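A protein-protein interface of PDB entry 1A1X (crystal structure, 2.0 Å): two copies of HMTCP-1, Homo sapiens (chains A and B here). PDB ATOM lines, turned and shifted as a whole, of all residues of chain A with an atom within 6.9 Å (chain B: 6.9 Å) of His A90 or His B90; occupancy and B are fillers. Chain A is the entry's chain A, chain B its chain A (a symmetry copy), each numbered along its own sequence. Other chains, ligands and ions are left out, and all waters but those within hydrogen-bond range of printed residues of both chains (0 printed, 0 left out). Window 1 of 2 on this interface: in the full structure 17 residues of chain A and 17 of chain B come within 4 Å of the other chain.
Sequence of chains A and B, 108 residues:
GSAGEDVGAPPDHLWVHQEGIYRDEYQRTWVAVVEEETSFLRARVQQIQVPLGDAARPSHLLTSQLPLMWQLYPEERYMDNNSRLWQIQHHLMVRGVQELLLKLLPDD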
ATOM      1  N   ARG A  44     -29.586 -25.481   0.832  1.00  0.00           N
ATOM      2  CA  ARG A  44     -28.204 -25.095   0.595  1.00  0.00           C
ATOM      3  C   ARG A  44     -27.409 -26.285   1.114  1.00  0.00           C
ATOM      4  O   ARG A  44     -27.536 -26.670   2.270  1.00  0.00           O
ATOM      5  CB  ARG A  44     -27.868 -23.813   1.355  1.00  0.00           C
ATOM      6  CG  ARG A  44     -26.515 -23.221   1.000  1.00  0.00           C
ATOM      7  CD  ARG A  44     -26.523 -21.717   1.213  1.00  0.00           C
ATOM      8  NE  ARG A  44     -26.884 -21.370   2.578  1.00  0.00           N
ATOM      9  CZ  ARG A  44     -26.030 -21.323   3.595  1.00  0.00           C
ATOM     10  NH1 ARG A  44     -24.747 -21.601   3.412  1.00  0.00           N
ATOM     11  NH2 ARG A  44     -26.465 -20.981   4.797  1.00  0.00           N
ATOM     12  N   GLN A  87     -33.990 -27.616  -8.927  1.00  0.00           N
ATOM     13  CA  GLN A  87     -33.123 -26.879  -9.836  1.00  0.00           C
ATOM     14  C   GLN A  87     -31.813 -26.493  -9.164  1.00  0.00           C
ATOM     15  O   GLN A  87     -31.821 -26.007  -8.039  1.00  0.00           O
ATOM     16  CB  GLN A  87     -33.836 -25.597 -10.293  1.00  0.00           C
ATOM     17  CG  GLN A  87     -33.051 -24.755 -11.289  1.00  0.00           C
ATOM     18  CD  GLN A  87     -32.886 -25.449 -12.632  1.00  0.00           C
ATOM     19  OE1 GLN A  87     -33.873 -25.806 -13.282  1.00  0.00           O
ATOM     20  NE2 GLN A  87     -31.638 -25.644 -13.056  1.00  0.00           N
ATOM     21  N   ILE A  88     -30.684 -26.735  -9.824  1.00  0.00           N
ATOM     22  CA  ILE A  88     -29.407 -26.319  -9.252  1.00  0.00           C
ATOM     23  C   ILE A  88     -29.292 -24.845  -9.641  1.00  0.00           C
ATOM     24  O   ILE A  88     -29.124 -24.528 -10.815  1.00  0.00           O
ATOM     25  CB  ILE A  88     -28.207 -27.096  -9.846  1.00  0.00           C
ATOM     26  CG1 ILE A  88     -28.262 -28.574  -9.447  1.00  0.00           C
ATOM     27  CG2 ILE A  88     -26.889 -26.492  -9.354  1.00  0.00           C
ATOM     28  CD1 ILE A  88     -27.229 -29.442 -10.177  1.00  0.00           C
ATOM     29  N   GLN A  89     -29.479 -23.947  -8.677  1.00  0.00           N
ATOM     30  CA  GLN A  89     -29.394 -22.511  -8.956  1.00  0.00           C
ATOM     31  C   GLN A  89     -27.952 -22.035  -9.002  1.00  0.00           C
ATOM     32  O   GLN A  89     -27.620 -21.087  -9.717  1.00  0.00           O
ATOM     33  CB  GLN A  89     -30.232 -21.717  -7.969  1.00  0.00           C
ATOM     34  CG  GLN A  89     -31.680 -22.144  -8.007  1.00  0.00           C
ATOM     35  CD  GLN A  89     -32.584 -21.109  -7.406  1.00  0.00           C
ATOM     36  OE1 GLN A  89     -32.690 -20.997  -6.193  1.00  0.00           O
ATOM     37  NE2 GLN A  89     -33.239 -20.334  -8.256  1.00  0.00           N
ATOM     38  N   HIS A  90     -27.106 -22.667  -8.194  1.00  0.00           N
ATOM     39  CA  HIS A  90     -25.676 -22.383  -8.237  1.00  0.00           C
ATOM     40  C   HIS A  90     -24.843 -23.496  -7.607  1.00  0.00           C
ATOM     41  O   HIS A  90     -25.320 -24.247  -6.752  1.00  0.00           O
ATOM     42  CB  HIS A  90     -25.310 -20.959  -7.759  1.00  0.00           C
ATOM     43  CG  HIS A  90     -25.202 -20.792  -6.276  1.00  0.00           C
ATOM     44  ND1 HIS A  90     -24.584 -21.713  -5.457  1.00  0.00           N
ATOM     45  CD2 HIS A  90     -25.572 -19.769  -5.474  1.00  0.00           C
ATOM     46  CE1 HIS A  90     -24.579 -21.264  -4.217  1.00  0.00           C
ATOM     47  NE2 HIS A  90     -25.175 -20.087  -4.200  1.00  0.00           N
ATOM     48  N   HIS A  91     -23.640 -23.658  -8.138  1.00  0.00           N
ATOM     49  CA  HIS A  91     -22.690 -24.661  -7.686  1.00  0.00           C
ATOM     50  C   HIS A  91     -21.348 -23.954  -7.688  1.00  0.00           C
ATOM     51  O   HIS A  91     -20.724 -23.772  -8.731  1.00  0.00           O
ATOM     52  CB  HIS A  91     -22.670 -25.841  -8.662  1.00  0.00           C
ATOM     53  CG  HIS A  91     -21.701 -26.925  -8.295  1.00  0.00           C
ATOM     54  ND1 HIS A  91     -21.242 -27.848  -9.209  1.00  0.00           N
ATOM     55  CD2 HIS A  91     -21.130 -27.252  -7.112  1.00  0.00           C
ATOM     56  CE1 HIS A  91     -20.432 -28.699  -8.604  1.00  0.00           C
ATOM     57  NE2 HIS A  91     -20.348 -28.360  -7.331  1.00  0.00           N
ATOM     58  N   LEU A  92     -20.915 -23.543  -6.505  1.00  0.00           N
ATOM     59  CA  LEU A  92     -19.671 -22.820  -6.381  1.00  0.00           C
ATOM     60  C   LEU A  92     -18.898 -23.117  -5.116  1.00  0.00           C
ATOM     61  O   LEU A  92     -19.336 -23.888  -4.259  1.00  0.00           O
ATOM     62  CB  LEU A  92     -19.921 -21.308  -6.517  1.00  0.00           C
ATOM     63  CG  LEU A  92     -21.287 -20.735  -6.126  1.00  0.00           C
ATOM     64  CD1 LEU A  92     -21.383 -20.580  -4.645  1.00  0.00           C
ATOM     65  CD2 LEU A  92     -21.506 -19.404  -6.793  1.00  0.00           C
ATOM     66  N   VAL A  94     -17.420 -21.588  -1.874  1.00  0.00           N
ATOM     67  CA  VAL A  94     -17.639 -20.445  -0.993  1.00  0.00           C
ATOM     68  C   VAL A  94     -16.788 -20.616   0.255  1.00  0.00           C
ATOM     69  O   VAL A  94     -16.979 -21.554   1.022  1.00  0.00           O
ATOM     70  CB  VAL A  94     -19.106 -20.310  -0.577  1.00  0.00           C
ATOM     71  CG1 VAL A  94     -19.275 -19.129   0.353  1.00  0.00           C
ATOM     72  CG2 VAL A  94     -19.971 -20.126  -1.782  1.00  0.00           C
ATOM     73  N   GLU A  99     -20.402 -25.712  -2.599  1.00  0.00           N
ATOM     74  CA  GLU A  99     -21.792 -25.480  -2.242  1.00  0.00           C
ATOM     75  C   GLU A  99     -22.799 -25.608  -3.382  1.00  0.00           C
ATOM     76  O   GLU A  99     -22.584 -25.096  -4.477  1.00  0.00           O
ATOM     77  CB  GLU A  99     -21.926 -24.092  -1.602  1.00  0.00           C
ATOM     78  CG  GLU A  99     -23.361 -23.669  -1.359  1.00  0.00           C
ATOM     79  CD  GLU A  99     -23.471 -22.279  -0.789  1.00  0.00           C
ATOM     80  OE1 GLU A  99     -23.150 -22.089   0.399  1.00  0.00           O
ATOM     81  OE2 GLU A  99     -23.898 -21.374  -1.518  1.00  0.00           O
ATOM     82  N   LEU A 100     -23.901 -26.302  -3.105  1.00  0.00           N
ATOM     83  CA  LEU A 100     -24.980 -26.459  -4.074  1.00  0.00           C
ATOM     84  C   LEU A 100     -26.152 -25.688  -3.523  1.00  0.00           C
ATOM     85  O   LEU A 100     -26.380 -25.704  -2.314  1.00  0.00           O
ATOM     86  CB  LEU A 100     -25.404 -27.922  -4.211  1.00  0.00           C
ATOM     87  CG  LEU A 100     -24.553 -28.904  -5.013  1.00  0.00           C
ATOM     88  CD1 LEU A 100     -25.077 -30.313  -4.787  1.00  0.00           C
ATOM     89  CD2 LEU A 100     -24.590 -28.544  -6.485  1.00  0.00           C
ATOM     90  N   LEU A 101     -26.826 -24.934  -4.387  1.00  0.00           N
ATOM     91  CA  LEU A 101     -28.021 -24.205  -3.986  1.00  0.00           C
ATOM     92  C   LEU A 101     -29.139 -24.791  -4.839  1.00  0.00           C
ATOM     93  O   LEU A 101     -29.193 -24.570  -6.057  1.00  0.00           O
ATOM     94  CB  LEU A 101     -27.899 -22.692  -4.211  1.00  0.00           C
ATOM     95  CG  LEU A 101     -29.146 -21.965  -3.680  1.00  0.00           C
ATOM     96  CD1 LEU A 101     -29.232 -22.127  -2.170  1.00  0.00           C
ATOM     97  CD2 LEU A 101     -29.136 -20.490  -4.079  1.00  0.00           C
ATOM     98  N   LEU A 102     -29.998 -25.577  -4.187  1.00  0.00           N
ATOM     99  CA  LEU A 102     -31.116 -26.267  -4.832  1.00  0.00           C
ATOM    100  C   LEU A 102     -32.468 -25.621  -4.575  1.00  0.00           C
ATOM    101  O   LEU A 102     -32.761 -25.194  -3.463  1.00  0.00           O
ATOM    102  CB  LEU A 102     -31.180 -27.717  -4.340  1.00  0.00           C
ATOM    103  CG  LEU A 102     -29.918 -28.561  -4.483  1.00  0.00           C
ATOM    104  CD1 LEU A 102     -30.146 -29.964  -3.913  1.00  0.00           C
ATOM    105  CD2 LEU A 102     -29.533 -28.624  -5.947  1.00  0.00           C
ATOM    106  N   ARG B  44     -21.713  -9.235  -3.660  1.00  0.00           N
ATOM    107  CA  ARG B  44     -23.099  -9.633  -3.475  1.00  0.00           C
ATOM    108  C   ARG B  44     -23.845  -8.307  -3.415  1.00  0.00           C
ATOM    109  O   ARG B  44     -23.548  -7.456  -2.585  1.00  0.00           O
ATOM    110  CB  ARG B  44     -23.259 -10.434  -2.184  1.00  0.00           C
ATOM    111  CG  ARG B  44     -24.628 -11.069  -2.016  1.00  0.00           C
ATOM    112  CD  ARG B  44     -24.529 -12.323  -1.165  1.00  0.00           C
ATOM    113  NE  ARG B  44     -23.939 -12.045   0.134  1.00  0.00           N
ATOM    114  CZ  ARG B  44     -24.614 -11.605   1.191  1.00  0.00           C
ATOM    115  NH1 ARG B  44     -25.921 -11.388   1.114  1.00  0.00           N
ATOM    116  NH2 ARG B  44     -23.978 -11.397   2.332  1.00  0.00           N
ATOM    117  N   GLN B  87     -19.030 -11.804 -13.927  1.00  0.00           N
ATOM    118  CA  GLN B  87     -20.005 -12.833 -14.263  1.00  0.00           C
ATOM    119  C   GLN B  87     -21.174 -12.832 -13.287  1.00  0.00           C
ATOM    120  O   GLN B  87     -20.965 -12.771 -12.082  1.00  0.00           O
ATOM    121  CB  GLN B  87     -19.327 -14.211 -14.215  1.00  0.00           C
ATOM    122  CG  GLN B  87     -20.230 -15.376 -14.594  1.00  0.00           C
ATOM    123  CD  GLN B  87     -20.637 -15.342 -16.059  1.00  0.00           C
ATOM    124  OE1 GLN B  87     -19.782 -15.347 -16.950  1.00  0.00           O
ATOM    125  NE2 GLN B  87     -21.944 -15.307 -16.318  1.00  0.00           N
ATOM    126  N   ILE B  88     -22.402 -12.864 -13.794  1.00  0.00           N
ATOM    127  CA  ILE B  88     -23.553 -12.935 -12.899  1.00  0.00           C
ATOM    128  C   ILE B  88     -23.673 -14.424 -12.572  1.00  0.00           C
ATOM    129  O   ILE B  88     -24.018 -15.221 -13.440  1.00  0.00           O
ATOM    130  CB  ILE B  88     -24.863 -12.456 -13.572  1.00  0.00           C
ATOM    131  CG1 ILE B  88     -24.800 -10.957 -13.883  1.00  0.00           C
ATOM    132  CG2 ILE B  88     -26.060 -12.730 -12.658  1.00  0.00           C
ATOM    133  CD1 ILE B  88     -25.970 -10.463 -14.743  1.00  0.00           C
ATOM    134  N   GLN B  89     -23.299 -14.810 -11.355  1.00  0.00           N
ATOM    135  CA  GLN B  89     -23.374 -16.217 -10.952  1.00  0.00           C
ATOM    136  C   GLN B  89     -24.785 -16.608 -10.549  1.00  0.00           C
ATOM    137  O   GLN B  89     -25.193 -17.762 -10.707  1.00  0.00           O
ATOM    138  CB  GLN B  89     -22.357 -16.524  -9.866  1.00  0.00           C
ATOM    139  CG  GLN B  89     -20.952 -16.213 -10.323  1.00  0.00           C
ATOM    140  CD  GLN B  89     -19.924 -16.909  -9.481  1.00  0.00           C
ATOM    141  OE1 GLN B  89     -19.620 -16.478  -8.378  1.00  0.00           O
ATOM    142  NE2 GLN B  89     -19.386 -18.004  -9.994  1.00  0.00           N
ATOM    143  N   HIS B  90     -25.513 -15.654  -9.979  1.00  0.00           N
ATOM    144  CA  HIS B  90     -26.918 -15.872  -9.659  1.00  0.00           C
ATOM    145  C   HIS B  90     -27.680 -14.565  -9.460  1.00  0.00           C
ATOM    146  O   HIS B  90     -27.100 -13.531  -9.116  1.00  0.00           O
ATOM    147  CB  HIS B  90     -27.149 -16.923  -8.549  1.00  0.00           C
ATOM    148  CG  HIS B  90     -27.009 -16.413  -7.149  1.00  0.00           C
ATOM    149  ND1 HIS B  90     -27.521 -15.202  -6.734  1.00  0.00           N
ATOM    150  CD2 HIS B  90     -26.476 -16.989  -6.050  1.00  0.00           C
ATOM    151  CE1 HIS B  90     -27.308 -15.056  -5.440  1.00  0.00           C
ATOM    152  NE2 HIS B  90     -26.672 -16.126  -5.001  1.00  0.00           N
ATOM    153  N   HIS B  91     -28.960 -14.609  -9.806  1.00  0.00           N
ATOM    154  CA  HIS B  91     -29.862 -13.473  -9.697  1.00  0.00           C
ATOM    155  C   HIS B  91     -31.157 -14.058  -9.169  1.00  0.00           C
ATOM    156  O   HIS B  91     -31.935 -14.657  -9.908  1.00  0.00           O
ATOM    157  CB  HIS B  91     -30.084 -12.847 -11.077  1.00  0.00           C
ATOM    158  CG  HIS B  91     -31.021 -11.676 -11.075  1.00  0.00           C
ATOM    159  ND1 HIS B  91     -31.656 -11.236 -12.216  1.00  0.00           N
ATOM    160  CD2 HIS B  91     -31.405 -10.838 -10.084  1.00  0.00           C
ATOM    161  CE1 HIS B  91     -32.390 -10.175 -11.927  1.00  0.00           C
ATOM    162  NE2 HIS B  91     -32.253  -9.913 -10.640  1.00  0.00           N
ATOM    163  N   LEU B  92     -31.377 -13.886  -7.874  1.00  0.00           N
ATOM    164  CA  LEU B  92     -32.558 -14.432  -7.244  1.00  0.00           C
ATOM    165  C   LEU B  92     -33.125 -13.577  -6.134  1.00  0.00           C
ATOM    166  O   LEU B  92     -32.584 -12.524  -5.790  1.00  0.00           O
ATOM    167  CB  LEU B  92     -32.274 -15.857  -6.735  1.00  0.00           C
ATOM    168  CG  LEU B  92     -30.842 -16.249  -6.358  1.00  0.00           C
ATOM    169  CD1 LEU B  92     -30.503 -15.736  -4.999  1.00  0.00           C
ATOM    170  CD2 LEU B  92     -30.684 -17.745  -6.394  1.00  0.00           C
ATOM    171  N   VAL B  94     -34.001 -13.458  -2.358  1.00  0.00           N
ATOM    172  CA  VAL B  94     -33.598 -14.101  -1.111  1.00  0.00           C
ATOM    173  C   VAL B  94     -34.241 -13.364   0.052  1.00  0.00           C
ATOM    174  O   VAL B  94     -33.966 -12.192   0.283  1.00  0.00           O
ATOM    175  CB  VAL B  94     -32.079 -14.094  -0.922  1.00  0.00           C
ATOM    176  CG1 VAL B  94     -31.717 -14.748   0.393  1.00  0.00           C
ATOM    177  CG2 VAL B  94     -31.413 -14.824  -2.043  1.00  0.00           C
ATOM    178  N   GLU B  99     -31.333 -10.196  -5.304  1.00  0.00           N
ATOM    179  CA  GLU B  99     -29.896 -10.299  -5.111  1.00  0.00           C
ATOM    180  C   GLU B  99     -29.093 -10.726  -6.336  1.00  0.00           C
ATOM    181  O   GLU B  99     -29.463 -11.661  -7.041  1.00  0.00           O
ATOM    182  CB  GLU B  99     -29.609 -11.265  -3.954  1.00  0.00           C
ATOM    183  CG  GLU B  99     -28.138 -11.591  -3.785  1.00  0.00           C
ATOM    184  CD  GLU B  99     -27.885 -12.589  -2.685  1.00  0.00           C
ATOM    185  OE1 GLU B  99     -28.001 -12.222  -1.502  1.00  0.00           O
ATOM    186  OE2 GLU B  99     -27.547 -13.738  -2.998  1.00  0.00           O
ATOM    187  N   LEU B 100     -27.988 -10.024  -6.577  1.00  0.00           N
ATOM    188  CA  LEU B 100     -27.087 -10.352  -7.676  1.00  0.00           C
ATOM    189  C   LEU B 100     -25.812 -10.844  -7.039  1.00  0.00           C
ATOM    190  O   LEU B 100     -25.393 -10.304  -6.016  1.00  0.00           O
ATOM    191  CB  LEU B 100     -26.746  -9.119  -8.512  1.00  0.00           C
ATOM    192  CG  LEU B 100     -27.752  -8.560  -9.516  1.00  0.00           C
ATOM    193  CD1 LEU B 100     -27.253  -7.218 -10.025  1.00  0.00           C
ATOM    194  CD2 LEU B 100     -27.940  -9.535 -10.662  1.00  0.00           C
ATOM    195  N   LEU B 101     -25.260 -11.928  -7.577  1.00  0.00           N
ATOM    196  CA  LEU B 101     -23.988 -12.449  -7.094  1.00  0.00           C
ATOM    197  C   LEU B 101     -23.045 -12.344  -8.287  1.00  0.00           C
ATOM    198  O   LEU B 101     -23.181 -13.082  -9.272  1.00  0.00           O
ATOM    199  CB  LEU B 101     -24.087 -13.900  -6.603  1.00  0.00           C
ATOM    200  CG  LEU B 101     -22.744 -14.365  -6.016  1.00  0.00           C
ATOM    201  CD1 LEU B 101     -22.422 -13.554  -4.769  1.00  0.00           C
ATOM    202  CD2 LEU B 101     -22.763 -15.862  -5.714  1.00  0.00           C
ATOM    203  N   LEU B 102     -22.123 -11.384  -8.198  1.00  0.00           N
ATOM    204  CA  LEU B 102     -21.150 -11.093  -9.253  1.00  0.00           C
ATOM    205  C   LEU B 102     -19.752 -11.610  -8.959  1.00  0.00           C
ATOM    206  O   LEU B 102     -19.267 -11.512  -7.837  1.00  0.00           O
ATOM    207  CB  LEU B 102     -21.063  -9.578  -9.470  1.00  0.00           C
ATOM    208  CG  LEU B 102     -22.363  -8.837  -9.765  1.00  0.00           C
ATOM    209  CD1 LEU B 102     -22.099  -7.337  -9.920  1.00  0.00           C
ATOM    210  CD2 LEU B 102     -22.982  -9.414 -11.022  1.00  0.00           C
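A ring nitrogen (NE2) of His A90 lies close to the side-chain carboxylate (OE2) of Glu A99. The backbone carbonyl oxygen (O) of His B90 lies within hydrogen-bond range of the backbone NH (N) of Leu B101, at 2.9 Å. N of Gln A89 is in hydrogen-bond range of O of Leu A101 (2.7 Å). N of Leu A101 lies within hydrogen-bond range of O of His A90, 2.9 Å away. The backbone carbonyl oxygen (O) of Leu B101 sits at hydrogen-bond distance from the backbone NH (N) of Gln B89, 2.7 Å away. The backbone NH (N) of Glu A99 sits at hydrogen-bond distance from the backbone carbonyl oxygen (O) of Leu A92 (2.7 Å).
Among the printed residues, merely in contact across the chains: His A90 with His B90 (3.0 Å), Leu A92 with Gln B89 (3.8 Å), Gln A89 with Leu B92 (3.8 Å), Leu A92 with Leu B101 (3.9 Å) and Leu A101 with Leu B92 (3.9 Å).
Of chain A, only His A90 (3.0 Å) comes within 4 Å of His B90. Of the printed residues of chain A, Leu B92 touches Gln A89 and Leu A101. Val B94 touches none of the printed residues of chain A. Printed residues of chain A within 4 Å of Leu B101: Leu A92 (3.9 Å). The nearest residue of chain B that does not touch His A90 is Gln B89 (4.4 Å).
Of the 12 printed residues of chain B, 4 touch a printed residue of chain A. Hydrophobic or aromatic side chains of chain B that line the printed part of chain A: His B90, Leu B92 and Leu B101. Along chain B the printed residues that touch a printed residue of chain A span positions 89 to 101. Along chain A the printed residues that touch a printed residue of chain B span positions 89 to 101. Among the printed residues, 5 pairs touch across the chains. Among the printed residues, no Asp or Glu carboxylate lies within 4 Å of a Lys or Arg side-chain nitrogen of the other chain.
Gln A89 touches Leu B92, and with the chains exchanged Leu A92 touches Gln B89. His B90 touches its own counterpart, His A90. Leu A92 touches Leu B101, and with the chains exchanged Leu A101 touches Leu B92. Of the 5 pairs that touch across the chains among the printed residues, 5 have their exchanged pair printed and touching as well.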
